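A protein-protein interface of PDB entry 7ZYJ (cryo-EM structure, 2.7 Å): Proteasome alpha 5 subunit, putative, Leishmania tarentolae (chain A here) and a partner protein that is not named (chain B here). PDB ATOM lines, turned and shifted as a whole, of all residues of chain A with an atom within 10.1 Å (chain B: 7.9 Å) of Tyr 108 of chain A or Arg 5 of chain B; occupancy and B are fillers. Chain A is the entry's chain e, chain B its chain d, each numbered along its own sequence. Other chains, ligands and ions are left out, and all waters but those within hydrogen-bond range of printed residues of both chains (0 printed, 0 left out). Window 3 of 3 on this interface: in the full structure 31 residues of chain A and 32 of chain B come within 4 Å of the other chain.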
ATOM      1  N   GLU A 107      24.516  20.683  27.260  1.00  0.00           N
ATOM      2  CA  GLU A 107      24.739  19.272  27.549  1.00  0.00           C
ATOM      3  C   GLU A 107      23.655  18.422  26.891  1.00  0.00           C
ATOM      4  O   GLU A 107      22.487  18.810  26.858  1.00  0.00           O
ATOM      5  CB  GLU A 107      24.770  19.031  29.060  1.00  0.00           C
ATOM      6  CG  GLU A 107      25.244  17.644  29.465  1.00  0.00           C
ATOM      7  CD  GLU A 107      26.707  17.407  29.150  1.00  0.00           C
ATOM      8  OE1 GLU A 107      27.011  16.957  28.026  1.00  0.00           O
ATOM      9  OE2 GLU A 107      27.555  17.670  30.029  1.00  0.00           O
ATOM     10  N   TYR A 108      24.045  17.259  26.367  1.00  0.00           N
ATOM     11  CA  TYR A 108      23.149  16.406  25.598  1.00  0.00           C
ATOM     12  C   TYR A 108      22.834  15.094  26.307  1.00  0.00           C
ATOM     13  O   TYR A 108      22.388  14.139  25.663  1.00  0.00           O
ATOM     14  CB  TYR A 108      23.743  16.134  24.217  1.00  0.00           C
ATOM     15  CG  TYR A 108      24.061  17.388  23.438  1.00  0.00           C
ATOM     16  CD1 TYR A 108      23.095  18.007  22.658  1.00  0.00           C
ATOM     17  CD2 TYR A 108      25.324  17.959  23.493  1.00  0.00           C
ATOM     18  CE1 TYR A 108      23.382  19.156  21.947  1.00  0.00           C
ATOM     19  CE2 TYR A 108      25.621  19.106  22.786  1.00  0.00           C
ATOM     20  CZ  TYR A 108      24.646  19.700  22.015  1.00  0.00           C
ATOM     21  OH  TYR A 108      24.939  20.844  21.310  1.00  0.00           O
ATOM     22  N   ASP A 109      23.064  15.024  27.618  1.00  0.00           N
ATOM     23  CA  ASP A 109      22.744  13.813  28.366  1.00  0.00           C
ATOM     24  C   ASP A 109      21.248  13.533  28.325  1.00  0.00           C
ATOM     25  O   ASP A 109      20.815  12.385  28.178  1.00  0.00           O
ATOM     26  CB  ASP A 109      23.224  13.951  29.812  1.00  0.00           C
ATOM     27  CG  ASP A 109      22.869  15.294  30.414  1.00  0.00           C
ATOM     28  OD1 ASP A 109      22.460  16.196  29.653  1.00  0.00           O
ATOM     29  OD2 ASP A 109      23.003  15.452  31.647  1.00  0.00           O
ATOM     30  N   ARG A 110      20.443  14.582  28.451  1.00  0.00           N
ATOM     31  CA  ARG A 110      18.997  14.458  28.526  1.00  0.00           C
ATOM     32  C   ARG A 110      18.339  15.160  27.343  1.00  0.00           C
ATOM     33  O   ARG A 110      18.842  16.163  26.830  1.00  0.00           O
ATOM     34  CB  ARG A 110      18.502  15.034  29.853  1.00  0.00           C
ATOM     35  CG  ARG A 110      18.677  16.536  29.978  1.00  0.00           C
ATOM     36  CD  ARG A 110      18.279  17.023  31.357  1.00  0.00           C
ATOM     37  NE  ARG A 110      19.224  16.537  32.356  1.00  0.00           N
ATOM     38  CZ  ARG A 110      19.077  16.669  33.666  1.00  0.00           C
ATOM     39  NH1 ARG A 110      18.046  17.312  34.184  1.00  0.00           N
ATOM     40  NH2 ARG A 110      19.997  16.154  34.479  1.00  0.00           N
ATOM     41  N   GLY A 111      17.212  14.611  26.907  1.00  0.00           N
ATOM     42  CA  GLY A 111      16.530  15.112  25.734  1.00  0.00           C
ATOM     43  C   GLY A 111      15.842  16.441  25.983  1.00  0.00           C
ATOM     44  O   GLY A 111      15.710  16.924  27.108  1.00  0.00           O
ATOM     45  N   VAL A 112      15.389  17.046  24.884  1.00  0.00           N
ATOM     46  CA  VAL A 112      14.726  18.341  24.959  1.00  0.00           C
ATOM     47  C   VAL A 112      13.252  18.229  25.332  1.00  0.00           C
ATOM     48  O   VAL A 112      12.634  19.244  25.688  1.00  0.00           O
ATOM     49  CB  VAL A 112      14.866  19.104  23.630  1.00  0.00           C
ATOM     50  CG1 VAL A 112      16.326  19.420  23.355  1.00  0.00           C
ATOM     51  CG2 VAL A 112      14.268  18.296  22.490  1.00  0.00           C
ATOM     52  N   THR A 114      12.228  16.089  27.767  1.00  0.00           N
ATOM     53  CA  THR A 114      12.202  15.413  29.054  1.00  0.00           C
ATOM     54  C   THR A 114      11.520  16.268  30.113  1.00  0.00           C
ATOM     55  O   THR A 114      11.542  17.501  30.062  1.00  0.00           O
ATOM     56  CB  THR A 114      13.619  15.068  29.511  1.00  0.00           C
ATOM     57  OG1 THR A 114      14.381  16.272  29.655  1.00  0.00           O
ATOM     58  CG2 THR A 114      14.295  14.169  28.497  1.00  0.00           C
ATOM     59  N   GLN A 123      13.996  22.253  29.046  1.00  0.00           N
ATOM     60  CA  GLN A 123      14.333  23.267  28.052  1.00  0.00           C
ATOM     61  C   GLN A 123      13.500  24.528  28.238  1.00  0.00           C
ATOM     62  O   GLN A 123      14.010  25.644  28.089  1.00  0.00           O
ATOM     63  CB  GLN A 123      14.153  22.703  26.644  1.00  0.00           C
ATOM     64  CG  GLN A 123      15.265  21.767  26.215  1.00  0.00           C
ATOM     65  CD  GLN A 123      16.591  22.480  26.047  1.00  0.00           C
ATOM     66  OE1 GLN A 123      16.760  23.294  25.141  1.00  0.00           O
ATOM     67  NE2 GLN A 123      17.540  22.178  26.925  1.00  0.00           N
ATOM     68  N   TYR A 126      14.838  26.377  31.228  1.00  0.00           N
ATOM     69  CA  TYR A 126      16.112  27.001  30.897  1.00  0.00           C
ATOM     70  C   TYR A 126      15.926  28.228  30.017  1.00  0.00           C
ATOM     71  O   TYR A 126      16.667  29.206  30.161  1.00  0.00           O
ATOM     72  CB  TYR A 126      17.035  25.997  30.203  1.00  0.00           C
ATOM     73  CG  TYR A 126      17.453  24.823  31.062  1.00  0.00           C
ATOM     74  CD1 TYR A 126      17.195  24.803  32.426  1.00  0.00           C
ATOM     75  CD2 TYR A 126      18.104  23.731  30.504  1.00  0.00           C
ATOM     76  CE1 TYR A 126      17.574  23.731  33.208  1.00  0.00           C
ATOM     77  CE2 TYR A 126      18.487  22.654  31.278  1.00  0.00           C
ATOM     78  CZ  TYR A 126      18.220  22.661  32.630  1.00  0.00           C
ATOM     79  OH  TYR A 126      18.600  21.591  33.406  1.00  0.00           O
ATOM     80  N   GLY A 224      10.899  20.682  19.019  1.00  0.00           N
ATOM     81  CA  GLY A 224      11.163  19.306  19.395  1.00  0.00           C
ATOM     82  C   GLY A 224      12.380  18.735  18.697  1.00  0.00           C
ATOM     83  O   GLY A 224      13.280  19.481  18.301  1.00  0.00           O
ATOM     84  N   GLU A 225      12.430  17.412  18.543  1.00  0.00           N
ATOM     85  CA  GLU A 225      13.537  16.760  17.854  1.00  0.00           C
ATOM     86  C   GLU A 225      13.107  15.712  16.836  1.00  0.00           C
ATOM     87  O   GLU A 225      13.869  15.448  15.898  1.00  0.00           O
ATOM     88  CB  GLU A 225      14.489  16.106  18.870  1.00  0.00           C
ATOM     89  CG  GLU A 225      15.781  15.564  18.273  1.00  0.00           C
ATOM     90  CD  GLU A 225      16.835  15.273  19.322  1.00  0.00           C
ATOM     91  OE1 GLU A 225      17.132  16.174  20.134  1.00  0.00           O
ATOM     92  OE2 GLU A 225      17.367  14.143  19.332  1.00  0.00           O
ATOM     93  N   SER A 226      11.920  15.126  16.967  1.00  0.00           N
ATOM     94  CA  SER A 226      11.461  14.081  16.053  1.00  0.00           C
ATOM     95  C   SER A 226      11.218  14.686  14.677  1.00  0.00           C
ATOM     96  O   SER A 226      10.393  15.589  14.518  1.00  0.00           O
ATOM     97  CB  SER A 226      10.198  13.422  16.594  1.00  0.00           C
ATOM     98  OG  SER A 226       9.736  12.406  15.720  1.00  0.00           O
ATOM     99  N   GLY A 227      11.938  14.190  13.674  1.00  0.00           N
ATOM    100  CA  GLY A 227      11.758  14.667  12.318  1.00  0.00           C
ATOM    101  C   GLY A 227      10.428  14.251  11.725  1.00  0.00           C
ATOM    102  O   GLY A 227       9.547  15.090  11.519  1.00  0.00           O
ATOM    103  N   GLY A 228      10.268  12.956  11.463  1.00  0.00           N
ATOM    104  CA  GLY A 228       9.017  12.428  10.955  1.00  0.00           C
ATOM    105  C   GLY A 228       8.520  13.104   9.695  1.00  0.00           C
ATOM    106  O   GLY A 228       9.117  12.963   8.623  1.00  0.00           O
ATOM    107  N   LYS A 231       9.494  19.379  10.052  1.00  0.00           N
ATOM    108  CA  LYS A 231      10.717  19.861  10.678  1.00  0.00           C
ATOM    109  C   LYS A 231      10.364  20.835  11.795  1.00  0.00           C
ATOM    110  O   LYS A 231       9.816  21.913  11.537  1.00  0.00           O
ATOM    111  CB  LYS A 231      11.619  20.528   9.644  1.00  0.00           C
ATOM    112  CG  LYS A 231      12.856  21.178  10.236  1.00  0.00           C
ATOM    113  CD  LYS A 231      13.773  20.148  10.870  1.00  0.00           C
ATOM    114  CE  LYS A 231      15.002  20.807  11.470  1.00  0.00           C
ATOM    115  NZ  LYS A 231      14.645  21.679  12.623  1.00  0.00           N
ATOM    116  N   LEU A 232      10.675  20.459  13.030  1.00  0.00           N
ATOM    117  CA  LEU A 232      10.406  21.282  14.197  1.00  0.00           C
ATOM    118  C   LEU A 232      11.664  22.035  14.608  1.00  0.00           C
ATOM    119  O   LEU A 232      12.765  21.776  14.116  1.00  0.00           O
ATOM    120  CB  LEU A 232       9.894  20.425  15.362  1.00  0.00           C
ATOM    121  CG  LEU A 232       8.493  19.830  15.220  1.00  0.00           C
ATOM    122  CD1 LEU A 232       8.157  18.963  16.424  1.00  0.00           C
ATOM    123  CD2 LEU A 232       7.458  20.928  15.039  1.00  0.00           C
ATOM    124  N   MET A 233      11.485  22.983  15.523  1.00  0.00           N
ATOM    125  CA  MET A 233      12.605  23.744  16.053  1.00  0.00           C
ATOM    126  C   MET A 233      13.373  22.914  17.071  1.00  0.00           C
ATOM    127  O   MET A 233      12.783  22.197  17.884  1.00  0.00           O
ATOM    128  CB  MET A 233      12.116  25.039  16.698  1.00  0.00           C
ATOM    129  CG  MET A 233      11.514  26.026  15.720  1.00  0.00           C
ATOM    130  SD  MET A 233      11.016  27.553  16.529  1.00  0.00           S
ATOM    131  CE  MET A 233       9.544  27.010  17.392  1.00  0.00           C
ATOM    132  N   SER A 234      14.701  23.020  17.027  1.00  0.00           N
ATOM    133  CA  SER A 234      15.549  22.261  17.937  1.00  0.00           C
ATOM    134  C   SER A 234      15.453  22.741  19.378  1.00  0.00           C
ATOM    135  O   SER A 234      15.913  22.031  20.278  1.00  0.00           O
ATOM    136  CB  SER A 234      17.005  22.325  17.468  1.00  0.00           C
ATOM    137  OG  SER A 234      17.603  23.557  17.830  1.00  0.00           O
ATOM    138  N   ARG A 235      14.872  23.912  19.621  1.00  0.00           N
ATOM    139  CA  ARG A 235      14.802  24.479  20.959  1.00  0.00           C
ATOM    140  C   ARG A 235      13.655  25.475  20.998  1.00  0.00           C
ATOM    141  O   ARG A 235      13.230  25.976  19.951  1.00  0.00           O
ATOM    142  CB  ARG A 235      16.123  25.167  21.337  1.00  0.00           C
ATOM    143  CG  ARG A 235      16.598  26.169  20.303  1.00  0.00           C
ATOM    144  CD  ARG A 235      17.668  27.086  20.862  1.00  0.00           C
ATOM    145  NE  ARG A 235      18.056  28.110  19.900  1.00  0.00           N
ATOM    146  CZ  ARG A 235      17.431  29.270  19.750  1.00  0.00           C
ATOM    147  NH1 ARG A 235      16.381  29.590  20.489  1.00  0.00           N
ATOM    148  NH2 ARG A 235      17.869  30.128  18.834  1.00  0.00           N
ATOM    149  N   SER B   2      16.155  12.068   7.916  1.00  0.00           N
ATOM    150  CA  SER B   2      17.522  12.574   7.916  1.00  0.00           C
ATOM    151  C   SER B   2      17.939  13.031   9.309  1.00  0.00           C
ATOM    152  O   SER B   2      17.107  13.166  10.204  1.00  0.00           O
ATOM    153  CB  SER B   2      17.667  13.726   6.918  1.00  0.00           C
ATOM    154  OG  SER B   2      17.198  14.943   7.472  1.00  0.00           O
ATOM    155  N   TYR B   3      19.238  13.265   9.480  1.00  0.00           N
ATOM    156  CA  TYR B   3      19.770  13.697  10.766  1.00  0.00           C
ATOM    157  C   TYR B   3      19.259  15.088  11.112  1.00  0.00           C
ATOM    158  O   TYR B   3      19.600  16.069  10.443  1.00  0.00           O
ATOM    159  CB  TYR B   3      21.296  13.679  10.724  1.00  0.00           C
ATOM    160  CG  TYR B   3      21.961  14.006  12.041  1.00  0.00           C
ATOM    161  CD1 TYR B   3      22.127  13.034  13.016  1.00  0.00           C
ATOM    162  CD2 TYR B   3      22.435  15.284  12.303  1.00  0.00           C
ATOM    163  CE1 TYR B   3      22.738  13.327  14.218  1.00  0.00           C
ATOM    164  CE2 TYR B   3      23.047  15.586  13.502  1.00  0.00           C
ATOM    165  CZ  TYR B   3      23.197  14.604  14.456  1.00  0.00           C
ATOM    166  OH  TYR B   3      23.806  14.900  15.652  1.00  0.00           O
ATOM    167  N   ASP B   4      18.439  15.174  12.157  1.00  0.00           N
ATOM    168  CA  ASP B   4      17.890  16.446  12.611  1.00  0.00           C
ATOM    169  C   ASP B   4      17.937  16.539  14.130  1.00  0.00           C
ATOM    170  O   ASP B   4      17.035  17.093  14.766  1.00  0.00           O
ATOM    171  CB  ASP B   4      16.465  16.648  12.091  1.00  0.00           C
ATOM    172  CG  ASP B   4      15.462  15.727  12.758  1.00  0.00           C
ATOM    173  OD1 ASP B   4      15.738  14.514  12.860  1.00  0.00           O
ATOM    174  OD2 ASP B   4      14.401  16.224  13.189  1.00  0.00           O
ATOM    175  N   ARG B   5      18.999  16.012  14.731  1.00  0.00           N
ATOM    176  CA  ARG B   5      19.148  16.083  16.177  1.00  0.00           C
ATOM    177  C   ARG B   5      19.336  17.527  16.624  1.00  0.00           C
ATOM    178  O   ARG B   5      19.989  18.324  15.945  1.00  0.00           O
ATOM    179  CB  ARG B   5      20.332  15.233  16.636  1.00  0.00           C
ATOM    180  CG  ARG B   5      20.438  15.091  18.147  1.00  0.00           C
ATOM    181  CD  ARG B   5      21.243  13.867  18.539  1.00  0.00           C
ATOM    182  NE  ARG B   5      21.300  13.697  19.987  1.00  0.00           N
ATOM    183  CZ  ARG B   5      22.266  14.174  20.760  1.00  0.00           C
ATOM    184  NH1 ARG B   5      23.276  14.866  20.259  1.00  0.00           N
ATOM    185  NH2 ARG B   5      22.218  13.950  22.071  1.00  0.00           N
ATOM    186  N   ALA B   6      18.755  17.862  17.772  1.00  0.00           N
ATOM    187  CA  ALA B   6      18.900  19.200  18.329  1.00  0.00           C
ATOM    188  C   ALA B   6      20.344  19.427  18.754  1.00  0.00           C
ATOM    189  O   ALA B   6      20.841  18.763  19.669  1.00  0.00           O
ATOM    190  CB  ALA B   6      17.953  19.386  19.512  1.00  0.00           C
ATOM    191  N   ILE B   7      21.016  20.361  18.091  1.00  0.00           N
ATOM    192  CA  ILE B   7      22.413  20.671  18.367  1.00  0.00           C
ATOM    193  C   ILE B   7      22.545  21.900  19.254  1.00  0.00           C
ATOM    194  O   ILE B   7      23.298  21.895  20.227  1.00  0.00           O
ATOM    195  CB  ILE B   7      23.190  20.844  17.043  1.00  0.00           C
ATOM    196  CG1 ILE B   7      23.346  19.494  16.343  1.00  0.00           C
ATOM    197  CG2 ILE B   7      24.547  21.483  17.294  1.00  0.00           C
ATOM    198  CD1 ILE B   7      24.193  19.546  15.092  1.00  0.00           C
ATOM    199  N   THR B   8      21.811  22.963  18.938  1.00  0.00           N
ATOM    200  CA  THR B   8      21.788  24.166  19.761  1.00  0.00           C
ATOM    201  C   THR B   8      20.665  24.022  20.780  1.00  0.00           C
ATOM    202  O   THR B   8      19.483  24.064  20.424  1.00  0.00           O
ATOM    203  CB  THR B   8      21.595  25.411  18.899  1.00  0.00           C
ATOM    204  OG1 THR B   8      22.589  25.439  17.867  1.00  0.00           O
ATOM    205  CG2 THR B   8      21.718  26.667  19.747  1.00  0.00           C
ATOM    206  N   VAL B   9      21.033  23.846  22.049  1.00  0.00           N
ATOM    207  CA  VAL B   9      20.074  23.643  23.124  1.00  0.00           C
ATOM    208  C   VAL B   9      20.416  24.580  24.272  1.00  0.00           C
ATOM    209  O   VAL B   9      21.542  25.066  24.397  1.00  0.00           O
ATOM    210  CB  VAL B   9      20.046  22.178  23.618  1.00  0.00           C
ATOM    211  CG1 VAL B   9      19.670  21.238  22.485  1.00  0.00           C
ATOM    212  CG2 VAL B   9      21.390  21.793  24.214  1.00  0.00           C
ATOM    213  N   PHE B  10      19.420  24.831  25.114  1.00  0.00           N
ATOM    214  CA  PHE B  10      19.602  25.706  26.261  1.00  0.00           C
ATOM    215  C   PHE B  10      20.365  24.996  27.371  1.00  0.00           C
ATOM    216  O   PHE B  10      20.327  23.769  27.501  1.00  0.00           O
ATOM    217  CB  PHE B  10      18.252  26.193  26.787  1.00  0.00           C
ATOM    218  CG  PHE B  10      17.716  27.388  26.058  1.00  0.00           C
ATOM    219  CD1 PHE B  10      18.211  28.653  26.321  1.00  0.00           C
ATOM    220  CD2 PHE B  10      16.720  27.248  25.108  1.00  0.00           C
ATOM    221  CE1 PHE B  10      17.720  29.756  25.653  1.00  0.00           C
ATOM    222  CE2 PHE B  10      16.226  28.348  24.436  1.00  0.00           C
ATOM    223  CZ  PHE B  10      16.727  29.603  24.709  1.00  0.00           C
ATOM    224  N   PHE B  17      25.067  27.232  24.435  1.00  0.00           N
ATOM    225  CA  PHE B  17      26.503  26.979  24.380  1.00  0.00           C
ATOM    226  C   PHE B  17      27.034  26.988  22.953  1.00  0.00           C
ATOM    227  O   PHE B  17      28.156  27.446  22.720  1.00  0.00           O
ATOM    228  CB  PHE B  17      26.829  25.654  25.065  1.00  0.00           C
ATOM    229  CG  PHE B  17      26.901  25.750  26.561  1.00  0.00           C
ATOM    230  CD1 PHE B  17      27.040  26.982  27.180  1.00  0.00           C
ATOM    231  CD2 PHE B  17      26.831  24.615  27.349  1.00  0.00           C
ATOM    232  CE1 PHE B  17      27.108  27.079  28.556  1.00  0.00           C
ATOM    233  CE2 PHE B  17      26.899  24.706  28.725  1.00  0.00           C
ATOM    234  CZ  PHE B  17      27.038  25.939  29.328  1.00  0.00           C
ATOM    235  N   GLN B  18      26.255  26.489  21.991  1.00  0.00           N
ATOM    236  CA  GLN B  18      26.714  26.491  20.605  1.00  0.00           C
ATOM    237  C   GLN B  18      26.901  27.911  20.083  1.00  0.00           C
ATOM    238  O   GLN B  18      27.879  28.196  19.383  1.00  0.00           O
ATOM    239  CB  GLN B  18      25.729  25.720  19.726  1.00  0.00           C
ATOM    240  CG  GLN B  18      25.809  24.213  19.886  1.00  0.00           C
ATOM    241  CD  GLN B  18      27.191  23.668  19.596  1.00  0.00           C
ATOM    242  OE1 GLN B  18      27.658  23.703  18.459  1.00  0.00           O
ATOM    243  NE2 GLN B  18      27.853  23.155  20.625  1.00  0.00           N
ATOM    244  N   TYR B  21      30.023  29.357  21.630  1.00  0.00           N
ATOM    245  CA  TYR B  21      31.223  28.791  21.027  1.00  0.00           C
ATOM    246  C   TYR B  21      31.456  29.343  19.626  1.00  0.00           C
ATOM    247  O   TYR B  21      32.606  29.567  19.232  1.00  0.00           O
ATOM    248  CB  TYR B  21      31.131  27.267  20.998  1.00  0.00           C
ATOM    249  CG  TYR B  21      31.005  26.629  22.365  1.00  0.00           C
ATOM    250  CD1 TYR B  21      31.369  27.321  23.514  1.00  0.00           C
ATOM    251  CD2 TYR B  21      30.521  25.337  22.507  1.00  0.00           C
ATOM    252  CE1 TYR B  21      31.249  26.746  24.763  1.00  0.00           C
ATOM    253  CE2 TYR B  21      30.401  24.751  23.752  1.00  0.00           C
ATOM    254  CZ  TYR B  21      30.768  25.459  24.875  1.00  0.00           C
ATOM    255  OH  TYR B  21      30.651  24.881  26.118  1.00  0.00           O
ATOM    256  N   SER B 121      17.909  25.193  13.943  1.00  0.00           N
ATOM    257  CA  SER B 121      17.608  24.104  13.029  1.00  0.00           C
ATOM    258  C   SER B 121      18.274  22.826  13.517  1.00  0.00           C
ATOM    259  O   SER B 121      19.470  22.816  13.824  1.00  0.00           O
ATOM    260  CB  SER B 121      18.076  24.430  11.609  1.00  0.00           C
ATOM    261  OG  SER B 121      19.489  24.387  11.517  1.00  0.00           O
ATOM    262  N   GLY B 122      17.493  21.751  13.592  1.00  0.00           N
ATOM    263  CA  GLY B 122      18.019  20.484  14.068  1.00  0.00           C
ATOM    264  C   GLY B 122      18.993  19.872  13.075  1.00  0.00           C
ATOM    265  O   GLY B 122      18.804  19.934  11.861  1.00  0.00           O
ATOM    266  N   GLY B 123      20.052  19.272  13.612  1.00  0.00           N
ATOM    267  CA  GLY B 123      21.050  18.633  12.781  1.00  0.00           C
ATOM    268  C   GLY B 123      22.075  19.563  12.179  1.00  0.00           C
ATOM    269  O   GLY B 123      22.811  19.151  11.279  1.00  0.00           O
ATOM    270  N   SER B 124      22.149  20.807  12.644  1.00  0.00           N
ATOM    271  CA  SER B 124      23.087  21.775  12.099  1.00  0.00           C
ATOM    272  C   SER B 124      23.614  22.670  13.209  1.00  0.00           C
ATOM    273  O   SER B 124      22.863  23.074  14.101  1.00  0.00           O
ATOM    274  CB  SER B 124      22.434  22.632  11.009  1.00  0.00           C
ATOM    275  OG  SER B 124      21.785  23.761  11.566  1.00  0.00           O
ATOM    276  N   ARG B 125      24.904  22.970  13.150  1.00  0.00           N
ATOM    277  CA  ARG B 125      25.536  23.899  14.070  1.00  0.00           C
ATOM    278  C   ARG B 125      25.442  25.321  13.536  1.00  0.00           C
ATOM    279  O   ARG B 125      25.305  25.535  12.328  1.00  0.00           O
ATOM    280  CB  ARG B 125      26.997  23.509  14.284  1.00  0.00           C
ATOM    281  CG  ARG B 125      27.825  23.502  13.018  1.00  0.00           C
ATOM    282  CD  ARG B 125      29.293  23.739  13.318  1.00  0.00           C
ATOM    283  NE  ARG B 125      30.096  23.755  12.101  1.00  0.00           N
ATOM    284  CZ  ARG B 125      30.252  24.815  11.322  1.00  0.00           C
ATOM    285  NH1 ARG B 125      29.679  25.972  11.607  1.00  0.00           N
ATOM    286  NH2 ARG B 125      31.003  24.713  10.230  1.00  0.00           N
ATOM    287  N   PRO B 126      25.505  26.320  14.412  1.00  0.00           N
ATOM    288  CA  PRO B 126      25.423  27.711  13.954  1.00  0.00           C
ATOM    289  C   PRO B 126      26.648  28.116  13.147  1.00  0.00           C
ATOM    290  O   PRO B 126      27.721  27.518  13.242  1.00  0.00           O
ATOM    291  CB  PRO B 126      25.332  28.515  15.256  1.00  0.00           C
ATOM    292  CG  PRO B 126      24.912  27.529  16.295  1.00  0.00           C
ATOM    293  CD  PRO B 126      25.515  26.230  15.881  1.00  0.00           C
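N of Ala 6 of chain B is in hydrogen-bond range of OE1 of Glu 225 of chain A (3.3 Å). The side-chain hydroxyl (OH) of Tyr 108 of chain A lies close to the backbone carbonyl oxygen (O) of Ile 7 of chain B (2.2 Å). The backbone carbonyl oxygen of Thr 8 of chain B lies within hydrogen-bond range of the side-chain hydroxyl of Ser 234 of chain A, at 3.2 Å. The side-chain amino group (NZ) of Lys 231 of chain A lies close to the backbone NH (N) of Gly 122 of chain B (3.0 Å). OD2 of Asp 4 of chain B lies close to N of Gly 227 of chain A (3.2 Å). The backbone carbonyl oxygen (O) of Glu 225 of chain A lies close to the side-chain carboxylate (OD2) of Asp 4 of chain B (2.9 Å). The backbone NH (N) of Phe 10 of chain B lies within hydrogen-bond range of the side-chain amide oxygen (OE1) of Gln 123 of chain A.
The backbone NH of Gly 123 of chain B lies within hydrogen-bond range of the backbone carbonyl oxygen of Arg 5 of chain B (2.5 Å). OG of Ser 124 of chain B lies within hydrogen-bond range of O of Ser 121 of chain B, at 3.4 Å.
Among the printed residues, pairs that only touch across the chains: Tyr 108 of chain A with Arg 5 of chain B (3.4 Å), Glu 225 of chain A with Arg 5 of chain B (3.4 Å), Ser 234 of chain A with Ala 6 of chain B (3.4 Å), Tyr 108 of chain A with Ala 6 of chain B (3.4 Å), Arg 235 of chain A with Thr 8 of chain B (3.6 Å), Tyr 126 of chain A with Phe 10 of chain B (3.6 Å), Tyr 108 of chain A with Gln 18 of chain B (3.8 Å), Gln 123 of chain A with Val 9 of chain B (3.8 Å), Ser 226 of chain A with Asp 4 of chain B (3.8 Å), Lys 231 of chain A with Ser 121 of chain B (3.9 Å), Val 112 of chain A with Val 9 of chain B (3.9 Å) and Ser 234 of chain A with Gly 122 of chain B (3.9 Å).
Printed residues of chain B within 4 Å of Tyr 108 of chain A: Arg 5 (3.4 Å), Ala 6 (3.4 Å), Ile 7 (2.2 Å) and Gln 18 (3.8 Å). Arg 110 of chain A touches none of the printed residues of chain B. Of the printed residues of chain B, Val 112 of chain A touches Val 9 (3.9 Å). Printed residues of chain B within 4 Å of Ser 226 of chain A: Asp 4 (3.8 Å). No residue of chain A comes within 4 Å of Tyr 3 of chain B. Of chain A, only Glu 225 (2.9 Å), Ser 226 (3.8 Å) and Gly 227 (3.2 Å) come within 4 Å of Asp 4 of chain B. Of chain A, only Tyr 108 (3.4 Å) and Glu 225 (3.4 Å) come within 4 Å of Arg 5 of chain B. Printed residues of chain A within 4 Å of Ala 6 of chain B: Tyr 108 (3.4 Å), Glu 225 (3.3 Å) and Ser 234 (3.4 Å). Of the printed residues of chain A, Gln 18 of chain B touches Tyr 108 (3.8 Å). Of the printed residues of chain A, Ser 121 of chain B touches Lys 231 (3.9 Å). Gly 122 of chain B touches two residues of chain A. Gly 123 of chain B touches none of the printed residues of chain A. Arg 125 of chain B touches none of the printed residues of chain A. The nearest printed residue of chain B that does not touch Val 112 of chain A is Ala 6 of chain B (4.2 Å).
Of the 18 printed residues of chain B, 10 touch a printed residue of chain A. Hydrophobic or aromatic side chains of chain B within 4 Å of the printed part of chain A: Ala 6, Val 9 and Phe 10. Among the printed residues, 19 pairs touch across the chains.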
